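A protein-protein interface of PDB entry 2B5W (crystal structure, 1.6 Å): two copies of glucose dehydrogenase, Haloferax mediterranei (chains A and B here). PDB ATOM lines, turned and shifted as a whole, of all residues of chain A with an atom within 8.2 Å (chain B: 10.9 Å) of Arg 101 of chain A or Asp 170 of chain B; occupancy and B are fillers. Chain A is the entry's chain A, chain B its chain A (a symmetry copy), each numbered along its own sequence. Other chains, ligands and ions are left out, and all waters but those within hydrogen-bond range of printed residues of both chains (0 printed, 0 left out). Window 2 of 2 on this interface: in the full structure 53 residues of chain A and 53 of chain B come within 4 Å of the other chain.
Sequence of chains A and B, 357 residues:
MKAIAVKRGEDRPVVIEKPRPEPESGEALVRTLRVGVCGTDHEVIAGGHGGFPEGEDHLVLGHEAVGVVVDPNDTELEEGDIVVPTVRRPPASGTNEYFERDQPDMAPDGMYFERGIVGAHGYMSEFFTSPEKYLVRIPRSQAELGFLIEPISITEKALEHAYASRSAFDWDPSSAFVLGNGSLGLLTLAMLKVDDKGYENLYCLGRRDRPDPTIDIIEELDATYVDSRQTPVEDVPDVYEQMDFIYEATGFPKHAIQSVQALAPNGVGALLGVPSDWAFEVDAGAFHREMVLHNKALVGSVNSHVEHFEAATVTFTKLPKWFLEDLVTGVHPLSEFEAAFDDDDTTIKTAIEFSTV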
ATOM      1  N   THR A  95      19.668  20.651   4.496  1.00  0.00           N
ATOM      2  CA  THR A  95      18.270  20.306   4.637  1.00  0.00           C
ATOM      3  C   THR A  95      17.632  21.102   5.780  1.00  0.00           C
ATOM      4  O   THR A  95      18.309  21.760   6.594  1.00  0.00           O
ATOM      5  CB  THR A  95      18.105  18.804   4.825  1.00  0.00           C
ATOM      6  OG1 THR A  95      16.730  18.422   4.621  1.00  0.00           O
ATOM      7  CG2 THR A  95      18.407  18.395   6.283  1.00  0.00           C
ATOM      8  N   ASN A  96      16.310  21.112   5.772  1.00  0.00           N
ATOM      9  CA  ASN A  96      15.527  21.799   6.786  1.00  0.00           C
ATOM     10  C   ASN A  96      14.157  21.115   6.897  1.00  0.00           C
ATOM     11  O   ASN A  96      13.892  20.177   6.170  1.00  0.00           O
ATOM     12  CB  ASN A  96      15.449  23.307   6.474  1.00  0.00           C
ATOM     13  CG  ASN A  96      14.776  23.610   5.125  1.00  0.00           C
ATOM     14  OD1 ASN A  96      13.754  23.024   4.817  1.00  0.00           O
ATOM     15  ND2 ASN A  96      15.318  24.577   4.381  1.00  0.00           N
ATOM     16  N   GLU A  97      13.308  21.587   7.807  1.00  0.00           N
ATOM     17  CA  GLU A  97      12.016  20.971   8.065  1.00  0.00           C
ATOM     18  C   GLU A  97      11.147  20.842   6.800  1.00  0.00           C
ATOM     19  O   GLU A  97      10.364  19.896   6.673  1.00  0.00           O
ATOM     20  CB  GLU A  97      11.252  21.775   9.125  1.00  0.00           C
ATOM     21  CG  GLU A  97      10.882  23.199   8.712  1.00  0.00           C
ATOM     22  CD  GLU A  97       9.975  23.858   9.720  1.00  0.00           C
ATOM     23  OE1 GLU A  97      10.464  24.774  10.386  1.00  0.00           O
ATOM     24  OE2 GLU A  97       8.797  23.454   9.859  1.00  0.00           O
ATOM     25  N   TYR A  98      11.271  21.805   5.900  1.00  0.00           N
ATOM     26  CA  TYR A  98      10.400  21.796   4.711  1.00  0.00           C
ATOM     27  C   TYR A  98      10.788  20.663   3.793  1.00  0.00           C
ATOM     28  O   TYR A  98       9.931  19.955   3.268  1.00  0.00           O
ATOM     29  CB  TYR A  98      10.406  23.154   4.019  1.00  0.00           C
ATOM     30  CG  TYR A  98       9.892  24.221   4.953  1.00  0.00           C
ATOM     31  CD1 TYR A  98      10.761  25.019   5.648  1.00  0.00           C
ATOM     32  CD2 TYR A  98       8.536  24.373   5.159  1.00  0.00           C
ATOM     33  CE1 TYR A  98      10.307  25.974   6.511  1.00  0.00           C
ATOM     34  CE2 TYR A  98       8.056  25.317   6.034  1.00  0.00           C
ATOM     35  CZ  TYR A  98       8.953  26.121   6.714  1.00  0.00           C
ATOM     36  OH  TYR A  98       8.503  27.090   7.586  1.00  0.00           O
ATOM     37  N   PHE A  99      12.088  20.446   3.607  1.00  0.00           N
ATOM     38  CA  PHE A  99      12.550  19.321   2.817  1.00  0.00           C
ATOM     39  C   PHE A  99      12.346  17.978   3.542  1.00  0.00           C
ATOM     40  O   PHE A  99      11.927  16.986   2.942  1.00  0.00           O
ATOM     41  CB  PHE A  99      14.013  19.533   2.381  1.00  0.00           C
ATOM     42  CG  PHE A  99      14.164  20.605   1.317  1.00  0.00           C
ATOM     43  CD1 PHE A  99      14.130  20.271  -0.009  1.00  0.00           C
ATOM     44  CD2 PHE A  99      14.242  21.934   1.646  1.00  0.00           C
ATOM     45  CE1 PHE A  99      14.223  21.248  -0.995  1.00  0.00           C
ATOM     46  CE2 PHE A  99      14.313  22.924   0.677  1.00  0.00           C
ATOM     47  CZ  PHE A  99      14.297  22.555  -0.677  1.00  0.00           C
ATOM     48  N   GLU A 100      12.626  17.945   4.845  1.00  0.00           N
ATOM     49  CA  GLU A 100      12.447  16.711   5.620  1.00  0.00           C
ATOM     50  C   GLU A 100      11.003  16.208   5.693  1.00  0.00           C
ATOM     51  O   GLU A 100      10.764  14.998   5.652  1.00  0.00           O
ATOM     52  CB  GLU A 100      13.007  16.910   7.047  1.00  0.00           C
ATOM     53  CG  GLU A 100      14.523  17.079   7.085  1.00  0.00           C
ATOM     54  CD  GLU A 100      15.275  15.883   6.513  1.00  0.00           C
ATOM     55  OE1 GLU A 100      14.977  14.738   6.907  1.00  0.00           O
ATOM     56  OE2 GLU A 100      16.160  16.092   5.659  1.00  0.00           O
ATOM     57  N   ARG A 101      10.054  17.150   5.684  1.00  0.00           N
ATOM     58  CA  ARG A 101       8.618  16.844   5.731  1.00  0.00           C
ATOM     59  C   ARG A 101       8.016  16.783   4.328  1.00  0.00           C
ATOM     60  O   ARG A 101       6.793  16.709   4.190  1.00  0.00           O
ATOM     61  CB  ARG A 101       7.874  17.923   6.522  1.00  0.00           C
ATOM     62  CG  ARG A 101       8.230  17.926   8.010  1.00  0.00           C
ATOM     63  CD  ARG A 101       7.553  19.056   8.787  1.00  0.00           C
ATOM     64  NE  ARG A 101       7.899  19.057  10.216  1.00  0.00           N
ATOM     65  CZ  ARG A 101       7.429  19.950  11.099  1.00  0.00           C
ATOM     66  NH1 ARG A 101       6.592  20.923  10.717  1.00  0.00           N
ATOM     67  NH2 ARG A 101       7.745  19.951  12.401  1.00  0.00           N
ATOM     68  N   ASP A 102       8.831  16.784   3.259  1.00  0.00           N
ATOM     69  CA  ASP A 102       8.341  16.619   1.873  1.00  0.00           C
ATOM     70  C   ASP A 102       7.393  17.733   1.486  1.00  0.00           C
ATOM     71  O   ASP A 102       6.401  17.494   0.773  1.00  0.00           O
ATOM     72  CB  ASP A 102       7.628  15.267   1.674  1.00  0.00           C
ATOM     73  CG  ASP A 102       8.492  14.109   2.016  1.00  0.00           C
ATOM     74  OD1 ASP A 102       9.584  13.995   1.443  1.00  0.00           O
ATOM     75  OD2 ASP A 102       8.145  13.251   2.856  1.00  0.00           O
ATOM     76  N   GLN A 103       7.645  18.934   1.983  1.00  0.00           N
ATOM     77  CA  GLN A 103       6.863  20.110   1.559  1.00  0.00           C
ATOM     78  C   GLN A 103       7.767  21.308   1.290  1.00  0.00           C
ATOM     79  O   GLN A 103       7.583  22.407   1.806  1.00  0.00           O
ATOM     80  CB  GLN A 103       5.705  20.430   2.534  1.00  0.00           C
ATOM     81  CG  GLN A 103       6.130  20.659   3.998  1.00  0.00           C
ATOM     82  CD  GLN A 103       4.959  20.969   4.935  1.00  0.00           C
ATOM     83  OE1 GLN A 103       5.124  21.669   5.936  1.00  0.00           O
ATOM     84  NE2 GLN A 103       3.783  20.449   4.606  1.00  0.00           N
ATOM     85  N   PRO A 104       8.771  21.122   0.425  1.00  0.00           N
ATOM     86  CA  PRO A 104       9.675  22.246   0.158  1.00  0.00           C
ATOM     87  C   PRO A 104       9.019  23.399  -0.586  1.00  0.00           C
ATOM     88  O   PRO A 104       9.527  24.500  -0.596  1.00  0.00           O
ATOM     89  CB  PRO A 104      10.784  21.605  -0.677  1.00  0.00           C
ATOM     90  CG  PRO A 104      10.187  20.494  -1.331  1.00  0.00           C
ATOM     91  CD  PRO A 104       9.162  19.921  -0.331  1.00  0.00           C
ATOM     92  N   ASP A 105       7.866  23.142  -1.190  1.00  0.00           N
ATOM     93  CA  ASP A 105       7.104  24.155  -1.858  1.00  0.00           C
ATOM     94  C   ASP A 105       6.528  25.173  -0.858  1.00  0.00           C
ATOM     95  O   ASP A 105       6.065  26.227  -1.251  1.00  0.00           O
ATOM     96  CB  ASP A 105       5.977  23.487  -2.650  1.00  0.00           C
ATOM     97  CG  ASP A 105       5.054  22.733  -1.763  1.00  0.00           C
ATOM     98  OD1 ASP A 105       5.459  21.665  -1.271  1.00  0.00           O
ATOM     99  OD2 ASP A 105       3.912  23.148  -1.507  1.00  0.00           O
ATOM    100  N   MET A 106       6.582  24.852   0.444  1.00  0.00           N
ATOM    101  CA  MET A 106       6.147  25.769   1.495  1.00  0.00           C
ATOM    102  C   MET A 106       7.347  26.480   2.167  1.00  0.00           C
ATOM    103  O   MET A 106       7.175  27.260   3.089  1.00  0.00           O
ATOM    104  CB  MET A 106       5.329  25.042   2.580  1.00  0.00           C
ATOM    105  CG  MET A 106       4.160  24.193   2.019  1.00  0.00           C
ATOM    106  SD  MET A 106       2.897  25.198   1.147  1.00  0.00           S
ATOM    107  CE  MET A 106       2.301  26.283   2.466  1.00  0.00           C
ATOM    108  N   LYS A 133      14.006  11.282  -5.554  1.00  0.00           N
ATOM    109  CA  LYS A 133      12.827  11.744  -4.843  1.00  0.00           C
ATOM    110  C   LYS A 133      12.203  12.992  -5.471  1.00  0.00           C
ATOM    111  O   LYS A 133      11.058  13.294  -5.200  1.00  0.00           O
ATOM    112  CB  LYS A 133      13.156  12.019  -3.376  1.00  0.00           C
ATOM    113  CG  LYS A 133      14.097  13.173  -3.139  1.00  0.00           C
ATOM    114  CD  LYS A 133      14.620  13.185  -1.676  1.00  0.00           C
ATOM    115  CE  LYS A 133      13.531  13.619  -0.709  1.00  0.00           C
ATOM    116  NZ  LYS A 133      13.984  13.643   0.735  1.00  0.00           N
ATOM    117  N   TYR A 134      12.981  13.697  -6.294  1.00  0.00           N
ATOM    118  CA  TYR A 134      12.531  14.893  -7.016  1.00  0.00           C
ATOM    119  C   TYR A 134      12.382  14.650  -8.515  1.00  0.00           C
ATOM    120  O   TYR A 134      12.203  15.616  -9.267  1.00  0.00           O
ATOM    121  CB  TYR A 134      13.475  16.078  -6.773  1.00  0.00           C
ATOM    122  CG  TYR A 134      13.656  16.412  -5.298  1.00  0.00           C
ATOM    123  CD1 TYR A 134      12.574  16.464  -4.449  1.00  0.00           C
ATOM    124  CD2 TYR A 134      14.915  16.582  -4.758  1.00  0.00           C
ATOM    125  CE1 TYR A 134      12.727  16.738  -3.106  1.00  0.00           C
ATOM    126  CE2 TYR A 134      15.068  16.862  -3.413  1.00  0.00           C
ATOM    127  CZ  TYR A 134      13.972  16.919  -2.587  1.00  0.00           C
ATOM    128  OH  TYR A 134      14.093  17.165  -1.206  1.00  0.00           O
ATOM    129  N   HIS A 161      -4.835  24.365  -2.388  1.00  0.00           N
ATOM    130  CA  HIS A 161      -4.876  25.255  -1.240  1.00  0.00           C
ATOM    131  C   HIS A 161      -6.092  26.180  -1.242  1.00  0.00           C
ATOM    132  O   HIS A 161      -6.727  26.371  -0.221  1.00  0.00           O
ATOM    133  CB  HIS A 161      -3.591  26.066  -1.117  1.00  0.00           C
ATOM    134  CG  HIS A 161      -2.411  25.245  -0.738  1.00  0.00           C
ATOM    135  ND1 HIS A 161      -1.797  25.367   0.495  1.00  0.00           N
ATOM    136  CD2 HIS A 161      -1.699  24.319  -1.421  1.00  0.00           C
ATOM    137  CE1 HIS A 161      -0.792  24.504   0.565  1.00  0.00           C
ATOM    138  NE2 HIS A 161      -0.695  23.873  -0.594  1.00  0.00           N
ATOM    139  N   HIS A 305       4.785  20.447  -5.614  1.00  0.00           N
ATOM    140  CA  HIS A 305       5.597  19.301  -5.259  1.00  0.00           C
ATOM    141  C   HIS A 305       5.051  18.019  -5.854  1.00  0.00           C
ATOM    142  O   HIS A 305       4.175  18.034  -6.723  1.00  0.00           O
ATOM    143  CB  HIS A 305       5.773  19.193  -3.732  1.00  0.00           C
ATOM    144  CG  HIS A 305       7.047  18.504  -3.343  1.00  0.00           C
ATOM    145  ND1 HIS A 305       8.269  18.851  -3.879  1.00  0.00           N
ATOM    146  CD2 HIS A 305       7.270  17.444  -2.520  1.00  0.00           C
ATOM    147  CE1 HIS A 305       9.199  18.058  -3.366  1.00  0.00           C
ATOM    148  NE2 HIS A 305       8.616  17.191  -2.545  1.00  0.00           N
ATOM    149  N   TYR B 163      -8.249  27.698   9.755  1.00  0.00           N
ATOM    150  CA  TYR B 163      -7.465  26.488   9.850  1.00  0.00           C
ATOM    151  C   TYR B 163      -7.704  25.595   8.640  1.00  0.00           C
ATOM    152  O   TYR B 163      -6.771  24.935   8.137  1.00  0.00           O
ATOM    153  CB  TYR B 163      -7.751  25.748  11.148  1.00  0.00           C
ATOM    154  CG  TYR B 163      -7.367  26.483  12.421  1.00  0.00           C
ATOM    155  CD1 TYR B 163      -6.620  27.658  12.394  1.00  0.00           C
ATOM    156  CD2 TYR B 163      -7.733  25.970  13.665  1.00  0.00           C
ATOM    157  CE1 TYR B 163      -6.278  28.297  13.581  1.00  0.00           C
ATOM    158  CE2 TYR B 163      -7.387  26.595  14.827  1.00  0.00           C
ATOM    159  CZ  TYR B 163      -6.654  27.762  14.780  1.00  0.00           C
ATOM    160  OH  TYR B 163      -6.308  28.390  15.985  1.00  0.00           O
ATOM    161  N   ALA B 164      -8.912  25.622   8.099  1.00  0.00           N
ATOM    162  CA  ALA B 164      -9.178  24.849   6.883  1.00  0.00           C
ATOM    163  C   ALA B 164      -8.274  25.308   5.746  1.00  0.00           C
ATOM    164  O   ALA B 164      -7.808  24.478   4.927  1.00  0.00           O
ATOM    165  CB  ALA B 164     -10.655  24.947   6.472  1.00  0.00           C
ATOM    166  N   SER B 165      -8.029  26.615   5.655  1.00  0.00           N
ATOM    167  CA  SER B 165      -7.166  27.142   4.607  1.00  0.00           C
ATOM    168  C   SER B 165      -5.753  26.613   4.641  1.00  0.00           C
ATOM    169  O   SER B 165      -5.055  26.739   3.623  1.00  0.00           O
ATOM    170  CB  SER B 165      -7.120  28.674   4.599  1.00  0.00           C
ATOM    171  OG  SER B 165      -6.227  29.166   5.601  1.00  0.00           O
ATOM    172  N   ARG B 166      -5.301  26.113   5.795  1.00  0.00           N
ATOM    173  CA  ARG B 166      -3.937  25.600   5.983  1.00  0.00           C
ATOM    174  C   ARG B 166      -3.905  24.061   5.932  1.00  0.00           C
ATOM    175  O   ARG B 166      -2.883  23.449   6.184  1.00  0.00           O
ATOM    176  CB  ARG B 166      -3.390  26.057   7.367  1.00  0.00           C
ATOM    177  CG  ARG B 166      -3.424  27.547   7.670  1.00  0.00           C
ATOM    178  CD  ARG B 166      -2.548  28.410   6.742  1.00  0.00           C
ATOM    179  NE  ARG B 166      -3.170  28.540   5.420  1.00  0.00           N
ATOM    180  CZ  ARG B 166      -2.497  28.862   4.326  1.00  0.00           C
ATOM    181  NH1 ARG B 166      -3.117  28.877   3.140  1.00  0.00           N
ATOM    182  NH2 ARG B 166      -1.197  29.135   4.388  1.00  0.00           N
ATOM    183  N   SER B 167      -5.027  23.427   5.615  1.00  0.00           N
ATOM    184  CA  SER B 167      -5.157  21.966   5.760  1.00  0.00           C
ATOM    185  C   SER B 167      -4.526  21.144   4.648  1.00  0.00           C
ATOM    186  O   SER B 167      -4.465  19.908   4.780  1.00  0.00           O
ATOM    187  CB  SER B 167      -6.627  21.561   5.947  1.00  0.00           C
ATOM    188  OG  SER B 167      -7.443  21.838   4.814  1.00  0.00           O
ATOM    189  N   ALA B 168      -4.077  21.786   3.585  1.00  0.00           N
ATOM    190  CA  ALA B 168      -3.416  21.092   2.479  1.00  0.00           C
ATOM    191  C   ALA B 168      -1.935  20.810   2.756  1.00  0.00           C
ATOM    192  O   ALA B 168      -1.283  20.106   1.982  1.00  0.00           O
ATOM    193  CB  ALA B 168      -3.607  21.849   1.167  1.00  0.00           C
ATOM    194  N   PHE B 169      -1.401  21.349   3.842  1.00  0.00           N
ATOM    195  CA  PHE B 169      -0.007  21.083   4.228  1.00  0.00           C
ATOM    196  C   PHE B 169       0.069  20.821   5.743  1.00  0.00           C
ATOM    197  O   PHE B 169      -0.915  20.899   6.458  1.00  0.00           O
ATOM    198  CB  PHE B 169       0.925  22.185   3.724  1.00  0.00           C
ATOM    199  CG  PHE B 169       0.789  23.490   4.447  1.00  0.00           C
ATOM    200  CD1 PHE B 169      -0.287  24.334   4.175  1.00  0.00           C
ATOM    201  CD2 PHE B 169       1.754  23.897   5.383  1.00  0.00           C
ATOM    202  CE1 PHE B 169      -0.422  25.564   4.847  1.00  0.00           C
ATOM    203  CE2 PHE B 169       1.636  25.109   6.022  1.00  0.00           C
ATOM    204  CZ  PHE B 169       0.552  25.939   5.785  1.00  0.00           C
ATOM    205  N   ASP B 170       1.260  20.469   6.216  1.00  0.00           N
ATOM    206  CA  ASP B 170       1.494  20.230   7.636  1.00  0.00           C
ATOM    207  C   ASP B 170       1.821  21.573   8.291  1.00  0.00           C
ATOM    208  O   ASP B 170       2.958  22.054   8.231  1.00  0.00           O
ATOM    209  CB  ASP B 170       2.616  19.201   7.844  1.00  0.00           C
ATOM    210  CG  ASP B 170       2.812  18.820   9.313  1.00  0.00           C
ATOM    211  OD1 ASP B 170       1.947  19.194  10.147  1.00  0.00           O
ATOM    212  OD2 ASP B 170       3.787  18.151   9.718  1.00  0.00           O
ATOM    213  N   TRP B 171       0.799  22.201   8.866  1.00  0.00           N
ATOM    214  CA  TRP B 171       0.949  23.496   9.490  1.00  0.00           C
ATOM    215  C   TRP B 171       0.941  23.242  11.003  1.00  0.00           C
ATOM    216  O   TRP B 171       0.014  22.632  11.551  1.00  0.00           O
ATOM    217  CB  TRP B 171      -0.224  24.395   9.112  1.00  0.00           C
ATOM    218  CG  TRP B 171      -0.151  25.837   9.555  1.00  0.00           C
ATOM    219  CD1 TRP B 171       0.853  26.752   9.308  1.00  0.00           C
ATOM    220  CD2 TRP B 171      -1.150  26.543  10.293  1.00  0.00           C
ATOM    221  NE1 TRP B 171       0.539  27.965   9.863  1.00  0.00           N
ATOM    222  CE2 TRP B 171      -0.699  27.873  10.458  1.00  0.00           C
ATOM    223  CE3 TRP B 171      -2.390  26.183  10.840  1.00  0.00           C
ATOM    224  CZ2 TRP B 171      -1.420  28.819  11.150  1.00  0.00           C
ATOM    225  CZ3 TRP B 171      -3.093  27.115  11.499  1.00  0.00           C
ATOM    226  CH2 TRP B 171      -2.617  28.427  11.640  1.00  0.00           C
ATOM    227  N   ASP B 172       1.978  23.706  11.661  1.00  0.00           N
ATOM    228  CA  ASP B 172       2.089  23.532  13.119  1.00  0.00           C
ATOM    229  C   ASP B 172       2.566  24.883  13.690  1.00  0.00           C
ATOM    230  O   ASP B 172       3.776  25.124  13.872  1.00  0.00           O
ATOM    231  CB  ASP B 172       3.048  22.408  13.444  1.00  0.00           C
ATOM    232  CG  ASP B 172       3.257  22.228  14.928  1.00  0.00           C
ATOM    233  OD1 ASP B 172       2.420  22.707  15.750  1.00  0.00           O
ATOM    234  OD2 ASP B 172       4.257  21.613  15.355  1.00  0.00           O
ATOM    235  N   PRO B 173       1.618  25.768  13.940  1.00  0.00           N
ATOM    236  CA  PRO B 173       1.940  27.135  14.339  1.00  0.00           C
ATOM    237  C   PRO B 173       2.372  27.255  15.788  1.00  0.00           C
ATOM    238  O   PRO B 173       1.985  26.432  16.637  1.00  0.00           O
ATOM    239  CB  PRO B 173       0.615  27.865  14.150  1.00  0.00           C
ATOM    240  CG  PRO B 173      -0.438  26.806  14.356  1.00  0.00           C
ATOM    241  CD  PRO B 173       0.159  25.570  13.834  1.00  0.00           C
ATOM    242  N   SER B 174       3.165  28.274  16.052  1.00  0.00           N
ATOM    243  CA  SER B 174       3.627  28.568  17.421  1.00  0.00           C
ATOM    244  C   SER B 174       3.241  29.924  17.946  1.00  0.00           C
ATOM    245  O   SER B 174       3.142  30.078  19.165  1.00  0.00           O
ATOM    246  CB  SER B 174       5.147  28.423  17.504  1.00  0.00           C
ATOM    247  OG  SER B 174       5.490  27.095  17.218  1.00  0.00           O
ATOM    248  N   LYS B 197      -4.084  23.602  18.693  1.00  0.00           N
ATOM    249  CA  LYS B 197      -2.887  23.881  17.906  1.00  0.00           C
ATOM    250  C   LYS B 197      -1.618  24.041  18.765  1.00  0.00           C
ATOM    251  O   LYS B 197      -0.487  23.966  18.238  1.00  0.00           O
ATOM    252  CB  LYS B 197      -3.042  25.155  17.066  1.00  0.00           C
ATOM    253  CG  LYS B 197      -4.079  25.093  15.944  1.00  0.00           C
ATOM    254  CD  LYS B 197      -3.573  24.412  14.730  1.00  0.00           C
ATOM    255  CE  LYS B 197      -4.655  24.231  13.674  1.00  0.00           C
ATOM    256  NZ  LYS B 197      -5.630  23.168  14.050  1.00  0.00           N
ATOM    257  N   GLU B 200       2.503  28.756  21.496  1.00  0.00           N
ATOM    258  CA  GLU B 200       3.510  28.977  22.541  1.00  0.00           C
ATOM    259  C   GLU B 200       3.597  30.441  22.932  1.00  0.00           C
ATOM    260  O   GLU B 200       3.830  30.749  24.105  1.00  0.00           O
ATOM    261  CB  GLU B 200       4.873  28.479  22.031  1.00  0.00           C
ATOM    262  CG  GLU B 200       4.885  26.986  21.699  1.00  0.00           C
ATOM    263  CD  GLU B 200       6.209  26.513  21.134  1.00  0.00           C
ATOM    264  OE1 GLU B 200       7.176  27.309  21.093  1.00  0.00           O
ATOM    265  OE2 GLU B 200       6.281  25.332  20.735  1.00  0.00           O
ATOM    266  N   ASP B 244       2.306  33.283  13.193  1.00  0.00           N
ATOM    267  CA  ASP B 244       1.720  32.211  12.393  1.00  0.00           C
ATOM    268  C   ASP B 244       0.235  32.382  12.163  1.00  0.00           C
ATOM    269  O   ASP B 244      -0.275  32.006  11.083  1.00  0.00           O
ATOM    270  CB  ASP B 244       1.965  30.878  13.028  1.00  0.00           C
ATOM    271  CG  ASP B 244       3.415  30.548  13.125  1.00  0.00           C
ATOM    272  OD1 ASP B 244       4.096  30.564  12.070  1.00  0.00           O
ATOM    273  OD2 ASP B 244       3.959  30.256  14.212  1.00  0.00           O
ATOM    274  N   PRO B 265       5.666  33.108   7.214  1.00  0.00           N
ATOM    275  CA  PRO B 265       5.408  32.330   6.003  1.00  0.00           C
ATOM    276  C   PRO B 265       4.415  31.204   6.289  1.00  0.00           C
ATOM    277  O   PRO B 265       4.476  30.565   7.362  1.00  0.00           O
ATOM    278  CB  PRO B 265       6.779  31.773   5.649  1.00  0.00           C
ATOM    279  CG  PRO B 265       7.693  32.859   6.131  1.00  0.00           C
ATOM    280  CD  PRO B 265       7.114  33.234   7.471  1.00  0.00           C
ATOM    281  N   ASN B 266       3.481  31.010   5.358  1.00  0.00           N
ATOM    282  CA  ASN B 266       2.490  29.944   5.429  1.00  0.00           C
ATOM    283  C   ASN B 266       1.387  30.230   6.452  1.00  0.00           C
ATOM    284  O   ASN B 266       0.544  29.387   6.665  1.00  0.00           O
ATOM    285  CB  ASN B 266       3.121  28.569   5.676  1.00  0.00           C
ATOM    286  CG  ASN B 266       4.299  28.312   4.780  1.00  0.00           C
ATOM    287  OD1 ASN B 266       4.313  28.764   3.630  1.00  0.00           O
ATOM    288  ND2 ASN B 266       5.304  27.621   5.295  1.00  0.00           N
ATOM    289  N   GLY B 267       1.389  31.413   7.030  1.00  0.00           N
ATOM    290  CA  GLY B 267       0.383  31.775   8.035  1.00  0.00           C
ATOM    291  C   GLY B 267      -0.959  32.175   7.420  1.00  0.00           C
ATOM    292  O   GLY B 267      -1.113  32.353   6.202  1.00  0.00           O
ATOM    293  N   ASN B 295       3.045  31.885   0.552  1.00  0.00           N
ATOM    294  CA  ASN B 295       1.924  30.970   0.695  1.00  0.00           C
ATOM    295  C   ASN B 295       1.012  31.356   1.856  1.00  0.00           C
ATOM    296  O   ASN B 295       0.684  30.493   2.691  1.00  0.00           O
ATOM    297  CB  ASN B 295       2.415  29.524   0.958  1.00  0.00           C
ATOM    298  CG  ASN B 295       3.296  28.929  -0.158  1.00  0.00           C
ATOM    299  OD1 ASN B 295       4.559  28.797  -0.005  1.00  0.00           O
ATOM    300  ND2 ASN B 295       2.668  28.510  -1.220  1.00  0.00           N
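O of Asn 266 of chain B sits at hydrogen-bond distance from NH2 of Arg 166 of chain B, at 2.9 Å.
The indole nitrogen (NE1) of Trp 171 of chain B lies within hydrogen-bond range of the backbone carbonyl oxygen (O) of Asn 266 of chain B (3.5 Å).
OE2 of Glu 97 of chain A is in salt-bridge range of NH1 of Arg 101 of chain A, 3.5 Å away.
NH2 of Arg 166 of chain B sits at hydrogen-bond distance from O of Asn 295 of chain B (2.9 Å).
The side-chain amide oxygen of Asn 96 of chain A is in hydrogen-bond range of the backbone NH of Tyr 98 of chain A (3.0 Å).
The backbone carbonyl oxygen (O) of Tyr 98 of chain A lies within hydrogen-bond range of the backbone NH (N) of Gln 103 of chain A (2.8 Å).
Among the printed residues, pairs that only touch across the chains: Gln 103 of chain A with Phe 169 of chain B (3.5 Å), Met 106 of chain A with Asn 295 of chain B (3.6 Å), His 161 of chain A with Phe 169 of chain B (3.6 Å), Met 106 of chain A with Phe 169 of chain B (3.7 Å), Tyr 98 of chain A with Asn 266 of chain B (3.7 Å), His 161 of chain A with Ala 168 of chain B (3.9 Å) and Arg 101 of chain A with Asp 170 of chain B (3.98 Å).
No residue of chain B comes within 4 Å of Glu 97 of chain A.
No residue of chain B comes within 4 Å of Glu 100 of chain A.
Of the printed residues of chain B, Arg 101 of chain A touches Asp 170 (3.98 Å).
No residue of chain B comes within 4 Å of Asp 102 of chain A.
Printed residues of chain B within 4 Å of Gln 103 of chain A: Phe 169 and Asp 170.
Of the printed residues of chain B, Met 106 of chain A touches Phe 169 (3.7 Å), Asn 266 (2.9 Å) and Asn 295 (3.6 Å).
Printed residues of chain B within 4 Å of His 161 of chain A: Ala 168 and Phe 169.
Asp 244 of chain B touches none of the printed residues of chain A.
Of the printed residues of chain A, Asn 266 of chain B touches Tyr 98 (3.7 Å) and Met 106 (2.9 Å).
Of the 16 printed residues of chain A, 6 touch a printed residue of chain B.
Printed residues of chain B that touch a printed residue of chain A: Ala 168, Phe 169, Asp 170, Asn 266 and Asn 295.
Among the printed residues, 10 pairs touch across the chains.
The backbone NH of Asp 170 of chain B lies close to the side-chain amide nitrogen of Gln 103 of chain A.
The side-chain amide oxygen of Asn 295 of chain B lies close to the backbone carbonyl oxygen of Asp 105 of chain A (3.2 Å).
O of Met 106 of chain A lies within hydrogen-bond range of ND2 of Asn 266 of chain B, 2.9 Å away.
No position is printed for both chains.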
